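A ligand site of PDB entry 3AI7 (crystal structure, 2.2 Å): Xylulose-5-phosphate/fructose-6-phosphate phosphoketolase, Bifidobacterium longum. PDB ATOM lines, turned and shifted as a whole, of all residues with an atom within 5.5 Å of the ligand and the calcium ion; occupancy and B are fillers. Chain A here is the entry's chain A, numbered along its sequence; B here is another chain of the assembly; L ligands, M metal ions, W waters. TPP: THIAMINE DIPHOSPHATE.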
ATOM      1  N   GLY A  66      -5.053  28.991  -5.087  1.00  0.00           N
ATOM      2  CA  GLY A  66      -5.985  29.026  -6.286  1.00  0.00           C
ATOM      3  C   GLY A  66      -6.515  30.414  -6.629  1.00  0.00           C
ATOM      4  O   GLY A  66      -6.307  30.935  -7.783  1.00  0.00           O
ATOM      5  N   THR A  67      -7.120  31.060  -5.624  1.00  0.00           N
ATOM      6  CA  THR A  67      -7.869  32.317  -5.841  1.00  0.00           C
ATOM      7  C   THR A  67      -6.837  33.451  -5.865  1.00  0.00           C
ATOM      8  O   THR A  67      -7.039  34.489  -6.417  1.00  0.00           O
ATOM      9  CB  THR A  67      -8.835  32.590  -4.651  1.00  0.00           C
ATOM     10  OG1 THR A  67      -9.776  33.595  -5.027  1.00  0.00           O
ATOM     11  CG2 THR A  67      -8.066  33.003  -3.316  1.00  0.00           C
ATOM     12  N   PRO A  95     -13.503  35.669  -1.608  1.00  0.00           N
ATOM     13  CA  PRO A  95     -12.677  34.439  -1.378  1.00  0.00           C
ATOM     14  C   PRO A  95     -11.665  34.731  -0.304  1.00  0.00           C
ATOM     15  O   PRO A  95     -10.471  34.910  -0.590  1.00  0.00           O
ATOM     16  CB  PRO A  95     -11.935  34.213  -2.715  1.00  0.00           C
ATOM     17  CG  PRO A  95     -12.725  35.153  -3.783  1.00  0.00           C
ATOM     18  CD  PRO A  95     -13.268  36.301  -2.930  1.00  0.00           C
ATOM     19  N   HIS A  97     -10.285  33.120   1.757  1.00  0.00           N
ATOM     20  CA  HIS A  97      -9.186  32.141   1.956  1.00  0.00           C
ATOM     21  C   HIS A  97      -7.989  32.560   1.105  1.00  0.00           C
ATOM     22  O   HIS A  97      -6.917  31.931   1.197  1.00  0.00           O
ATOM     23  CB  HIS A  97      -9.616  30.727   1.557  1.00  0.00           C
ATOM     24  CG  HIS A  97     -10.362  30.698   0.244  1.00  0.00           C
ATOM     25  ND1 HIS A  97     -11.683  31.126   0.122  1.00  0.00           N
ATOM     26  CD2 HIS A  97      -9.977  30.303  -0.994  1.00  0.00           C
ATOM     27  CE1 HIS A  97     -12.086  30.989  -1.127  1.00  0.00           C
ATOM     28  NE2 HIS A  97     -11.060  30.528  -1.845  1.00  0.00           N
ATOM     29  N   GLY A 154     -14.470  36.494   5.037  1.00  0.00           N
ATOM     30  CA  GLY A 154     -14.698  35.567   4.014  1.00  0.00           C
ATOM     31  C   GLY A 154     -14.396  34.133   4.357  1.00  0.00           C
ATOM     32  O   GLY A 154     -14.057  33.374   3.456  1.00  0.00           O
ATOM     33  N   GLY A 155     -14.494  33.734   5.619  1.00  0.00           N
ATOM     34  CA  GLY A 155     -14.293  32.333   5.982  1.00  0.00           C
ATOM     35  C   GLY A 155     -15.488  31.461   5.629  1.00  0.00           C
ATOM     36  O   GLY A 155     -15.354  30.421   4.962  1.00  0.00           O
ATOM     37  N   GLU A 156     -16.671  31.889   6.072  1.00  0.00           N
ATOM     38  CA  GLU A 156     -17.928  31.311   5.633  1.00  0.00           C
ATOM     39  C   GLU A 156     -18.402  32.147   4.446  1.00  0.00           C
ATOM     40  O   GLU A 156     -18.724  33.357   4.605  1.00  0.00           O
ATOM     41  CB  GLU A 156     -18.985  31.453   6.750  1.00  0.00           C
ATOM     42  CG  GLU A 156     -20.298  30.739   6.458  1.00  0.00           C
ATOM     43  CD  GLU A 156     -21.145  30.641   7.736  1.00  0.00           C
ATOM     44  OE1 GLU A 156     -20.761  29.890   8.687  1.00  0.00           O
ATOM     45  OE2 GLU A 156     -22.176  31.347   7.795  1.00  0.00           O
ATOM     46  N   LEU A 157     -18.516  31.519   3.296  1.00  0.00           N
ATOM     47  CA  LEU A 157     -18.741  32.254   2.065  1.00  0.00           C
ATOM     48  C   LEU A 157     -20.182  32.612   1.997  1.00  0.00           C
ATOM     49  O   LEU A 157     -21.033  31.885   2.578  1.00  0.00           O
ATOM     50  CB  LEU A 157     -18.409  31.348   0.906  1.00  0.00           C
ATOM     51  CG  LEU A 157     -16.916  31.004   0.864  1.00  0.00           C
ATOM     52  CD1 LEU A 157     -16.694  29.956  -0.284  1.00  0.00           C
ATOM     53  CD2 LEU A 157     -16.139  32.271   0.600  1.00  0.00           C
ATOM     54  N   GLY A 181     -16.491  35.063  -5.159  1.00  0.00           N
ATOM     55  CA  GLY A 181     -15.999  33.802  -5.794  1.00  0.00           C
ATOM     56  C   GLY A 181     -17.081  33.267  -6.724  1.00  0.00           C
ATOM     57  O   GLY A 181     -18.261  33.467  -6.470  1.00  0.00           O
ATOM     58  N   ASP A 182     -16.704  32.525  -7.763  1.00  0.00           N
ATOM     59  CA  ASP A 182     -17.771  31.901  -8.559  1.00  0.00           C
ATOM     60  C   ASP A 182     -18.417  30.702  -7.840  1.00  0.00           C
ATOM     61  O   ASP A 182     -19.643  30.418  -8.059  1.00  0.00           O
ATOM     62  CB  ASP A 182     -17.367  31.636 -10.021  1.00  0.00           C
ATOM     63  CG  ASP A 182     -16.082  30.812 -10.201  1.00  0.00           C
ATOM     64  OD1 ASP A 182     -15.308  30.611  -9.248  1.00  0.00           O
ATOM     65  OD2 ASP A 182     -15.895  30.314 -11.326  1.00  0.00           O
ATOM     66  N   GLY A 183     -17.671  30.080  -6.932  1.00  0.00           N
ATOM     67  CA  GLY A 183     -18.213  29.021  -6.027  1.00  0.00           C
ATOM     68  C   GLY A 183     -19.109  29.733  -5.025  1.00  0.00           C
ATOM     69  O   GLY A 183     -20.295  29.350  -4.855  1.00  0.00           O
ATOM     70  N   GLU A 184     -18.572  30.760  -4.360  1.00  0.00           N
ATOM     71  CA  GLU A 184     -19.355  31.530  -3.445  1.00  0.00           C
ATOM     72  C   GLU A 184     -20.729  31.952  -4.059  1.00  0.00           C
ATOM     73  O   GLU A 184     -21.750  31.964  -3.389  1.00  0.00           O
ATOM     74  CB  GLU A 184     -18.593  32.747  -2.929  1.00  0.00           C
ATOM     75  CG  GLU A 184     -19.472  33.726  -2.100  1.00  0.00           C
ATOM     76  CD  GLU A 184     -18.677  34.877  -1.480  1.00  0.00           C
ATOM     77  OE1 GLU A 184     -17.626  35.277  -2.071  1.00  0.00           O
ATOM     78  OE2 GLU A 184     -19.085  35.375  -0.374  1.00  0.00           O
ATOM     79  N   ALA A 185     -20.731  32.309  -5.325  1.00  0.00           N
ATOM     80  CA  ALA A 185     -22.006  32.728  -5.982  1.00  0.00           C
ATOM     81  C   ALA A 185     -23.018  31.623  -6.058  1.00  0.00           C
ATOM     82  O   ALA A 185     -24.201  31.907  -6.337  1.00  0.00           O
ATOM     83  CB  ALA A 185     -21.777  33.336  -7.376  1.00  0.00           C
ATOM     84  N   THR A 187     -24.004  29.983  -3.365  1.00  0.00           N
ATOM     85  CA  THR A 187     -24.639  29.978  -2.055  1.00  0.00           C
ATOM     86  C   THR A 187     -25.952  30.790  -2.128  1.00  0.00           C
ATOM     87  O   THR A 187     -26.062  31.736  -2.895  1.00  0.00           O
ATOM     88  CB  THR A 187     -23.802  30.584  -0.883  1.00  0.00           C
ATOM     89  OG1 THR A 187     -23.710  31.980  -1.127  1.00  0.00           O
ATOM     90  CG2 THR A 187     -22.420  30.022  -0.757  1.00  0.00           C
ATOM     91  N   HIS A 213     -15.363  36.711  -9.764  1.00  0.00           N
ATOM     92  CA  HIS A 213     -14.056  36.122  -9.919  1.00  0.00           C
ATOM     93  C   HIS A 213     -14.269  34.742 -10.553  1.00  0.00           C
ATOM     94  O   HIS A 213     -14.234  33.681  -9.904  1.00  0.00           O
ATOM     95  CB  HIS A 213     -13.359  36.003  -8.562  1.00  0.00           C
ATOM     96  CG  HIS A 213     -11.921  35.581  -8.684  1.00  0.00           C
ATOM     97  ND1 HIS A 213     -11.121  35.364  -7.587  1.00  0.00           N
ATOM     98  CD2 HIS A 213     -11.179  35.264  -9.757  1.00  0.00           C
ATOM     99  CE1 HIS A 213      -9.917  34.960  -7.986  1.00  0.00           C
ATOM    100  NE2 HIS A 213      -9.929  34.901  -9.308  1.00  0.00           N
ATOM    101  N   ASN A 215     -13.039  32.156 -12.048  1.00  0.00           N
ATOM    102  CA  ASN A 215     -11.847  31.355 -12.310  1.00  0.00           C
ATOM    103  C   ASN A 215     -12.164  29.910 -12.590  1.00  0.00           C
ATOM    104  O   ASN A 215     -11.252  29.084 -12.838  1.00  0.00           O
ATOM    105  CB  ASN A 215     -10.806  31.496 -11.201  1.00  0.00           C
ATOM    106  CG  ASN A 215     -11.301  31.010  -9.897  1.00  0.00           C
ATOM    107  OD1 ASN A 215     -12.267  30.247  -9.836  1.00  0.00           O
ATOM    108  ND2 ASN A 215     -10.625  31.388  -8.819  1.00  0.00           N
ATOM    109  N   GLY A 216     -13.465  29.604 -12.580  1.00  0.00           N
ATOM    110  CA  GLY A 216     -13.938  28.338 -13.198  1.00  0.00           C
ATOM    111  C   GLY A 216     -14.108  27.136 -12.278  1.00  0.00           C
ATOM    112  O   GLY A 216     -14.661  26.099 -12.699  1.00  0.00           O
ATOM    113  N   TYR A 217     -13.548  27.225 -11.062  1.00  0.00           N
ATOM    114  CA  TYR A 217     -13.541  26.095 -10.140  1.00  0.00           C
ATOM    115  C   TYR A 217     -13.759  26.501  -8.740  1.00  0.00           C
ATOM    116  O   TYR A 217     -13.455  27.659  -8.350  1.00  0.00           O
ATOM    117  CB  TYR A 217     -12.184  25.348 -10.224  1.00  0.00           C
ATOM    118  CG  TYR A 217     -11.994  24.870 -11.606  1.00  0.00           C
ATOM    119  CD1 TYR A 217     -12.551  23.662 -11.978  1.00  0.00           C
ATOM    120  CD2 TYR A 217     -11.429  25.706 -12.579  1.00  0.00           C
ATOM    121  CE1 TYR A 217     -12.471  23.210 -13.291  1.00  0.00           C
ATOM    122  CE2 TYR A 217     -11.318  25.273 -13.937  1.00  0.00           C
ATOM    123  CZ  TYR A 217     -11.840  24.007 -14.289  1.00  0.00           C
ATOM    124  OH  TYR A 217     -11.821  23.514 -15.595  1.00  0.00           O
ATOM    125  N   LYS A 218     -14.250  25.552  -7.952  1.00  0.00           N
ATOM    126  CA  LYS A 218     -14.325  25.700  -6.495  1.00  0.00           C
ATOM    127  C   LYS A 218     -13.268  24.683  -5.901  1.00  0.00           C
ATOM    128  O   LYS A 218     -12.144  24.617  -6.385  1.00  0.00           O
ATOM    129  CB  LYS A 218     -15.803  25.590  -5.978  1.00  0.00           C
ATOM    130  CG  LYS A 218     -16.778  24.621  -6.689  1.00  0.00           C
ATOM    131  CD  LYS A 218     -18.192  24.704  -6.154  1.00  0.00           C
ATOM    132  CE  LYS A 218     -19.081  23.565  -6.684  1.00  0.00           C
ATOM    133  NZ  LYS A 218     -19.711  23.866  -7.988  1.00  0.00           N
ATOM    134  N   ILE A 219     -13.610  23.882  -4.915  1.00  0.00           N
ATOM    135  CA  ILE A 219     -12.606  23.044  -4.330  1.00  0.00           C
ATOM    136  C   ILE A 219     -12.281  21.859  -5.245  1.00  0.00           C
ATOM    137  O   ILE A 219     -11.088  21.542  -5.561  1.00  0.00           O
ATOM    138  CB  ILE A 219     -13.035  22.467  -2.982  1.00  0.00           C
ATOM    139  CG1 ILE A 219     -13.217  23.584  -1.909  1.00  0.00           C
ATOM    140  CG2 ILE A 219     -11.948  21.466  -2.505  1.00  0.00           C
ATOM    141  CD1 ILE A 219     -13.592  23.014  -0.469  1.00  0.00           C
ATOM    142  N   THR A 223     -17.517  25.389 -11.568  1.00  0.00           N
ATOM    143  CA  THR A 223     -18.568  26.192 -11.010  1.00  0.00           C
ATOM    144  C   THR A 223     -19.651  26.330 -12.054  1.00  0.00           C
ATOM    145  O   THR A 223     -19.366  26.482 -13.260  1.00  0.00           O
ATOM    146  CB  THR A 223     -18.006  27.568 -10.630  1.00  0.00           C
ATOM    147  OG1 THR A 223     -17.258  28.049 -11.738  1.00  0.00           O
ATOM    148  CG2 THR A 223     -17.027  27.422  -9.444  1.00  0.00           C
ATOM    149  N   LYS A 300      -7.917  29.476 -12.711  1.00  0.00           N
ATOM    150  CA  LYS A 300      -7.694  29.465 -11.306  1.00  0.00           C
ATOM    151  C   LYS A 300      -6.222  29.083 -11.118  1.00  0.00           C
ATOM    152  O   LYS A 300      -5.647  28.300 -11.895  1.00  0.00           O
ATOM    153  CB  LYS A 300      -8.633  28.473 -10.639  1.00  0.00           C
ATOM    154  CG  LYS A 300      -8.392  28.289  -9.177  1.00  0.00           C
ATOM    155  CD  LYS A 300      -9.495  27.417  -8.570  1.00  0.00           C
ATOM    156  CE  LYS A 300      -9.530  27.598  -7.051  1.00  0.00           C
ATOM    157  NZ  LYS A 300     -10.875  27.147  -6.496  1.00  0.00           N
ATOM    158  N   HIS A 320      -6.541  24.749  -5.952  1.00  0.00           N
ATOM    159  CA  HIS A 320      -7.340  25.484  -4.959  1.00  0.00           C
ATOM    160  C   HIS A 320      -6.575  25.810  -3.680  1.00  0.00           C
ATOM    161  O   HIS A 320      -6.564  26.914  -3.182  1.00  0.00           O
ATOM    162  CB  HIS A 320      -8.580  24.664  -4.599  1.00  0.00           C
ATOM    163  CG  HIS A 320      -9.388  25.264  -3.513  1.00  0.00           C
ATOM    164  ND1 HIS A 320     -10.005  26.480  -3.647  1.00  0.00           N
ATOM    165  CD2 HIS A 320      -9.615  24.857  -2.234  1.00  0.00           C
ATOM    166  CE1 HIS A 320     -10.596  26.797  -2.509  1.00  0.00           C
ATOM    167  NE2 HIS A 320     -10.388  25.821  -1.638  1.00  0.00           N
ATOM    168  N   PRO B 435     -21.687  19.976  -0.273  1.00  0.00           N
ATOM    169  CA  PRO B 435     -21.468  21.307  -0.819  1.00  0.00           C
ATOM    170  C   PRO B 435     -19.997  21.480  -1.257  1.00  0.00           C
ATOM    171  O   PRO B 435     -19.266  22.312  -0.698  1.00  0.00           O
ATOM    172  CB  PRO B 435     -21.870  22.229   0.367  1.00  0.00           C
ATOM    173  CG  PRO B 435     -21.542  21.386   1.554  1.00  0.00           C
ATOM    174  CD  PRO B 435     -21.497  19.944   1.189  1.00  0.00           C
ATOM    175  N   ASP B 436     -19.572  20.675  -2.233  1.00  0.00           N
ATOM    176  CA  ASP B 436     -18.219  20.725  -2.803  1.00  0.00           C
ATOM    177  C   ASP B 436     -17.237  20.146  -1.814  1.00  0.00           C
ATOM    178  O   ASP B 436     -16.065  20.460  -1.825  1.00  0.00           O
ATOM    179  CB  ASP B 436     -17.881  22.164  -3.198  1.00  0.00           C
ATOM    180  CG  ASP B 436     -16.530  22.331  -3.953  1.00  0.00           C
ATOM    181  OD1 ASP B 436     -16.112  21.508  -4.846  1.00  0.00           O
ATOM    182  OD2 ASP B 436     -15.882  23.359  -3.635  1.00  0.00           O
ATOM    183  N   GLU B 437     -17.712  19.241  -0.964  1.00  0.00           N
ATOM    184  CA  GLU B 437     -16.875  18.684   0.090  1.00  0.00           C
ATOM    185  C   GLU B 437     -16.874  17.162   0.199  1.00  0.00           C
ATOM    186  O   GLU B 437     -16.253  16.637   1.103  1.00  0.00           O
ATOM    187  CB  GLU B 437     -17.289  19.254   1.459  1.00  0.00           C
ATOM    188  CG  GLU B 437     -17.160  20.773   1.550  1.00  0.00           C
ATOM    189  CD  GLU B 437     -17.936  21.352   2.744  1.00  0.00           C
ATOM    190  OE1 GLU B 437     -18.374  20.555   3.591  1.00  0.00           O
ATOM    191  OE2 GLU B 437     -18.104  22.590   2.849  1.00  0.00           O
ATOM    192  N   LEU B 477     -22.173  24.554  -4.183  1.00  0.00           N
ATOM    193  CA  LEU B 477     -21.620  25.142  -2.974  1.00  0.00           C
ATOM    194  C   LEU B 477     -22.761  25.884  -2.321  1.00  0.00           C
ATOM    195  O   LEU B 477     -22.888  27.104  -2.441  1.00  0.00           O
ATOM    196  CB  LEU B 477     -20.394  26.010  -3.274  1.00  0.00           C
ATOM    197  CG  LEU B 477     -19.640  26.870  -2.256  1.00  0.00           C
ATOM    198  CD1 LEU B 477     -19.961  26.676  -0.736  1.00  0.00           C
ATOM    199  CD2 LEU B 477     -18.081  27.119  -2.583  1.00  0.00           C
ATOM    200  N   GLU B 479     -25.046  24.733   1.326  1.00  0.00           N
ATOM    201  CA  GLU B 479     -25.656  23.898   2.340  1.00  0.00           C
ATOM    202  C   GLU B 479     -27.190  23.895   2.207  1.00  0.00           C
ATOM    203  O   GLU B 479     -27.802  22.866   2.480  1.00  0.00           O
ATOM    204  CB  GLU B 479     -25.212  24.333   3.774  1.00  0.00           C
ATOM    205  CG  GLU B 479     -23.684  24.080   4.018  1.00  0.00           C
ATOM    206  CD  GLU B 479     -22.777  25.165   3.368  1.00  0.00           C
ATOM    207  OE1 GLU B 479     -23.313  26.165   2.808  1.00  0.00           O
ATOM    208  OE2 GLU B 479     -21.527  24.966   3.323  1.00  0.00           O
ATOM    209  N   TYR B 501     -18.527  20.367   6.516  1.00  0.00           N
ATOM    210  CA  TYR B 501     -17.641  20.809   7.518  1.00  0.00           C
ATOM    211  C   TYR B 501     -18.562  21.192   8.641  1.00  0.00           C
ATOM    212  O   TYR B 501     -19.658  21.826   8.439  1.00  0.00           O
ATOM    213  CB  TYR B 501     -16.881  22.081   7.093  1.00  0.00           C
ATOM    214  CG  TYR B 501     -15.873  21.856   5.990  1.00  0.00           C
ATOM    215  CD1 TYR B 501     -15.620  20.583   5.506  1.00  0.00           C
ATOM    216  CD2 TYR B 501     -15.191  22.945   5.402  1.00  0.00           C
ATOM    217  CE1 TYR B 501     -14.669  20.352   4.448  1.00  0.00           C
ATOM    218  CE2 TYR B 501     -14.254  22.750   4.364  1.00  0.00           C
ATOM    219  CZ  TYR B 501     -14.004  21.455   3.883  1.00  0.00           C
ATOM    220  OH  TYR B 501     -13.086  21.251   2.871  1.00  0.00           O
ATOM    221  N   PHE B 504     -19.963  24.833   9.242  1.00  0.00           N
ATOM    222  CA  PHE B 504     -20.930  25.375   8.318  1.00  0.00           C
ATOM    223  C   PHE B 504     -22.262  24.625   8.329  1.00  0.00           C
ATOM    224  O   PHE B 504     -23.191  25.030   7.590  1.00  0.00           O
ATOM    225  CB  PHE B 504     -20.376  25.555   6.887  1.00  0.00           C
ATOM    226  CG  PHE B 504     -19.004  26.293   6.848  1.00  0.00           C
ATOM    227  CD1 PHE B 504     -18.771  27.401   7.650  1.00  0.00           C
ATOM    228  CD2 PHE B 504     -18.010  25.850   6.037  1.00  0.00           C
ATOM    229  CE1 PHE B 504     -17.554  28.029   7.668  1.00  0.00           C
ATOM    230  CE2 PHE B 504     -16.745  26.463   6.063  1.00  0.00           C
ATOM    231  CZ  PHE B 504     -16.532  27.563   6.847  1.00  0.00           C
ATOM    232  N   VAL B 507     -25.077  26.843   8.814  1.00  0.00           N
ATOM    233  CA  VAL B 507     -25.706  27.615   7.731  1.00  0.00           C
ATOM    234  C   VAL B 507     -27.207  27.136   7.597  1.00  0.00           C
ATOM    235  O   VAL B 507     -28.092  27.896   7.303  1.00  0.00           O
ATOM    236  CB  VAL B 507     -24.989  27.369   6.431  1.00  0.00           C
ATOM    237  CG1 VAL B 507     -25.872  27.714   5.181  1.00  0.00           C
ATOM    238  CG2 VAL B 507     -23.567  28.078   6.404  1.00  0.00           C
ATOM    239  N   HIS B 553     -13.843  28.623  11.025  1.00  0.00           N
ATOM    240  CA  HIS B 553     -14.240  27.285  10.754  1.00  0.00           C
ATOM    241  C   HIS B 553     -14.371  26.450  12.042  1.00  0.00           C
ATOM    242  O   HIS B 553     -14.342  25.250  11.962  1.00  0.00           O
ATOM    243  CB  HIS B 553     -13.120  26.653   9.898  1.00  0.00           C
ATOM    244  CG  HIS B 553     -13.130  27.081   8.466  1.00  0.00           C
ATOM    245  ND1 HIS B 553     -13.016  28.401   8.076  1.00  0.00           N
ATOM    246  CD2 HIS B 553     -13.251  26.360   7.330  1.00  0.00           C
ATOM    247  CE1 HIS B 553     -13.062  28.463   6.748  1.00  0.00           C
ATOM    248  NE2 HIS B 553     -13.195  27.239   6.286  1.00  0.00           N
HETATM  249  N1' TPP L   1     -19.407  26.413   2.749  1.00  0.00           N
HETATM  250  C2' TPP L   1     -19.369  27.689   3.106  1.00  0.00           C
HETATM  251  CM2 TPP L   1     -20.664  28.456   3.388  1.00  0.00           C
HETATM  252  N3' TPP L   1     -18.152  28.310   3.239  1.00  0.00           N
HETATM  253  C4' TPP L   1     -16.991  27.639   2.973  1.00  0.00           C
HETATM  254  N4' TPP L   1     -15.786  28.282   3.175  1.00  0.00           N
HETATM  255  C5' TPP L   1     -17.035  26.303   2.595  1.00  0.00           C
HETATM  256  C6' TPP L   1     -18.274  25.733   2.443  1.00  0.00           C
HETATM  257  C7' TPP L   1     -15.781  25.471   2.288  1.00  0.00           C
HETATM  258  N3  TPP L   1     -15.062  26.163   1.173  1.00  0.00           N
HETATM  259  C2  TPP L   1     -13.980  26.955   1.433  1.00  0.00           C
HETATM  260  S1  TPP L   1     -13.317  27.601  -0.097  1.00  0.00           S
HETATM  261  C5  TPP L   1     -14.549  26.695  -1.035  1.00  0.00           C
HETATM  262  C4  TPP L   1     -15.376  26.003  -0.154  1.00  0.00           C
HETATM  263  CM4 TPP L   1     -16.445  25.088  -0.629  1.00  0.00           C
HETATM  264  C6  TPP L   1     -14.515  26.849  -2.560  1.00  0.00           C
HETATM  265  C7  TPP L   1     -14.959  28.282  -2.886  1.00  0.00           C
HETATM  266  O7  TPP L   1     -14.628  28.534  -4.255  1.00  0.00           O
HETATM  267  PA  TPP L   1     -14.712  30.009  -4.904  1.00  0.00           P
HETATM  268  O1A TPP L   1     -15.882  30.889  -4.325  1.00  0.00           O
HETATM  269  O2A TPP L   1     -14.820  29.721  -6.568  1.00  0.00           O
HETATM  270  O3A TPP L   1     -13.265  30.620  -4.471  1.00  0.00           O
HETATM  271  PB  TPP L   1     -11.880  30.412  -5.305  1.00  0.00           P
HETATM  272  O1B TPP L   1     -12.002  29.501  -6.541  1.00  0.00           O
HETATM  273  O2B TPP L   1     -11.575  32.017  -5.914  1.00  0.00           O
HETATM  274  O3B TPP L   1     -10.593  29.798  -4.363  1.00  0.00           O
HETATM  275 CA    CA M   1     -13.586  29.860  -8.088  1.00  0.00          CA
HETATM  276  O   HOH W   1     -10.905  27.420   2.782  1.00  0.00           O
HETATM  277  O   HOH W   2     -13.526  32.103  -7.604  1.00  0.00           O
HETATM  278  O   HOH W   3     -13.090  25.898   3.893  1.00  0.00           O
HETATM  279  O   HOH W   4      -8.099  29.214  -3.731  1.00  0.00           O
HETATM  280  O   HOH W   5     -15.190  33.175  -2.672  1.00  0.00           O
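Water W2 lies within hydrogen-bond range of O2B of the ligand, O of His 213, N of Asp 182 and ND2 of Asn 215.
Water W4 lies within hydrogen-bond range of an oxygen (O3B) of the ligand (2.6 Å), the backbone carbonyl oxygen of His 320 (2.8 Å), the backbone NH of Thr 67 (2.8 Å) and the backbone NH of Gly 66 (3.3 Å).
Water W5 lies within hydrogen-bond range of an oxygen (O1A) of the ligand, the side-chain carboxylate (OE1) of Glu 184 and the backbone NH (N) of Gly 181.
The nearest printed residue that does not touch the calcium ion is Lys 300 (4.2 Å).
An oxygen (O2A) of the ligand is bound to the calcium ion, at 2.0 Å.
OD1 of Asp 182 is bound to the calcium ion (2.2 Å).
The calcium ion is bound by O of Tyr 217 (2.2 Å).
OD1 of Asn 215 binds the calcium ion, at 2.2 Å.
The calcium ion is bound by an oxygen (O1B) of the ligand, 2.2 Å away.
Water W2 is bound to the calcium ion, 2.3 Å away.
OG1 of Thr 67 sits at hydrogen-bond distance from O2B of the ligand, 2.6 Å away.
OE2 of Glu 479 of chain B is in hydrogen-bond range of N1' of the ligand (2.6 Å).
O of Gly 155 is in hydrogen-bond range of N4' of the ligand (2.8 Å).
The side-chain amino group of Lys 300 is in salt-bridge range of an oxygen (O3B) of the ligand, 3.4 Å away.
A ring nitrogen (ND1) of His 320 sits at hydrogen-bond distance from an oxygen (O3B) of the ligand (3.4 Å).
An oxygen (O3B) of the ligand lies within hydrogen-bond range of a ring nitrogen (NE2) of His 97 (2.7 Å).
The backbone NH of Gly 183 is in hydrogen-bond range of an oxygen (O1A) of the ligand (3.3 Å).
The backbone NH of Glu 184 lies within hydrogen-bond range of an oxygen (O1A) of the ligand, at 2.7 Å.
A nitrogen (N3') of the ligand lies within hydrogen-bond range of the backbone NH (N) of Leu 157 (3.2 Å).
ND1 of His 213 sits close to OG1 of Thr 67.
The side-chain carboxylate (OE1) of Glu 184 is in hydrogen-bond range of the backbone NH (N) of Gly 181 (3.3 Å).
N of Asp 182 lies close to O of His 213 (3.5 Å).
The side-chain amino group of Lys 300 lies within hydrogen-bond range of a ring nitrogen (ND1) of His 320.
The side-chain carboxylate (OD2) of Asp 436 of chain B sits at hydrogen-bond distance from the backbone NH (N) of Ile 219, 2.7 Å away.
NZ of Lys 300 is in hydrogen-bond range of O of Lys 218, 2.8 Å away.
OG1 of Thr 223 sits at hydrogen-bond distance from OD2 of Asp 182 (2.7 Å).
OE1 of Glu 437 of chain B is in hydrogen-bond range of N of Tyr 501 of chain B (2.9 Å).
Merely in contact with the ligand: Pro 95 (3.9 Å), Glu 156 (3.8 Å), Gly 181 (3.3 Å), His 213 (3.8 Å), Lys 218 (3.6 Å), Ile 219 (3.5 Å), Pro 435 of chain B (3.96 Å), Asp 436 of chain B (3.5 Å), Glu 437 of chain B (3.2 Å), Leu 477 of chain B (3.3 Å), Tyr 501 of chain B (3.7 Å) and Phe 504 of chain B (3.3 Å).
Hydrophobic or aromatic side chains within 4 Å of the ligand: Pro 95, His 97, Leu 157, His 213, Ile 219, His 320, Leu 477 of chain B, Tyr 501 of chain B and Phe 504 of chain B.
24 residues have an atom within 4 Å of the ligand: Thr 67, Pro 95, His 97, Gly 155, Glu 156, Leu 157, Gly 181, Asp 182, Gly 183, Glu 184, His 213, Asn 215, Tyr 217, Lys 218, Ile 219, Lys 300, His 320, Pro 435 of chain B, Asp 436 of chain B, Glu 437 of chain B, Leu 477 of chain B, Glu 479 of chain B, Tyr 501 of chain B and Phe 504 of chain B.
Along chain A the residues within 4 Å of the ligand span positions 67 to 320.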
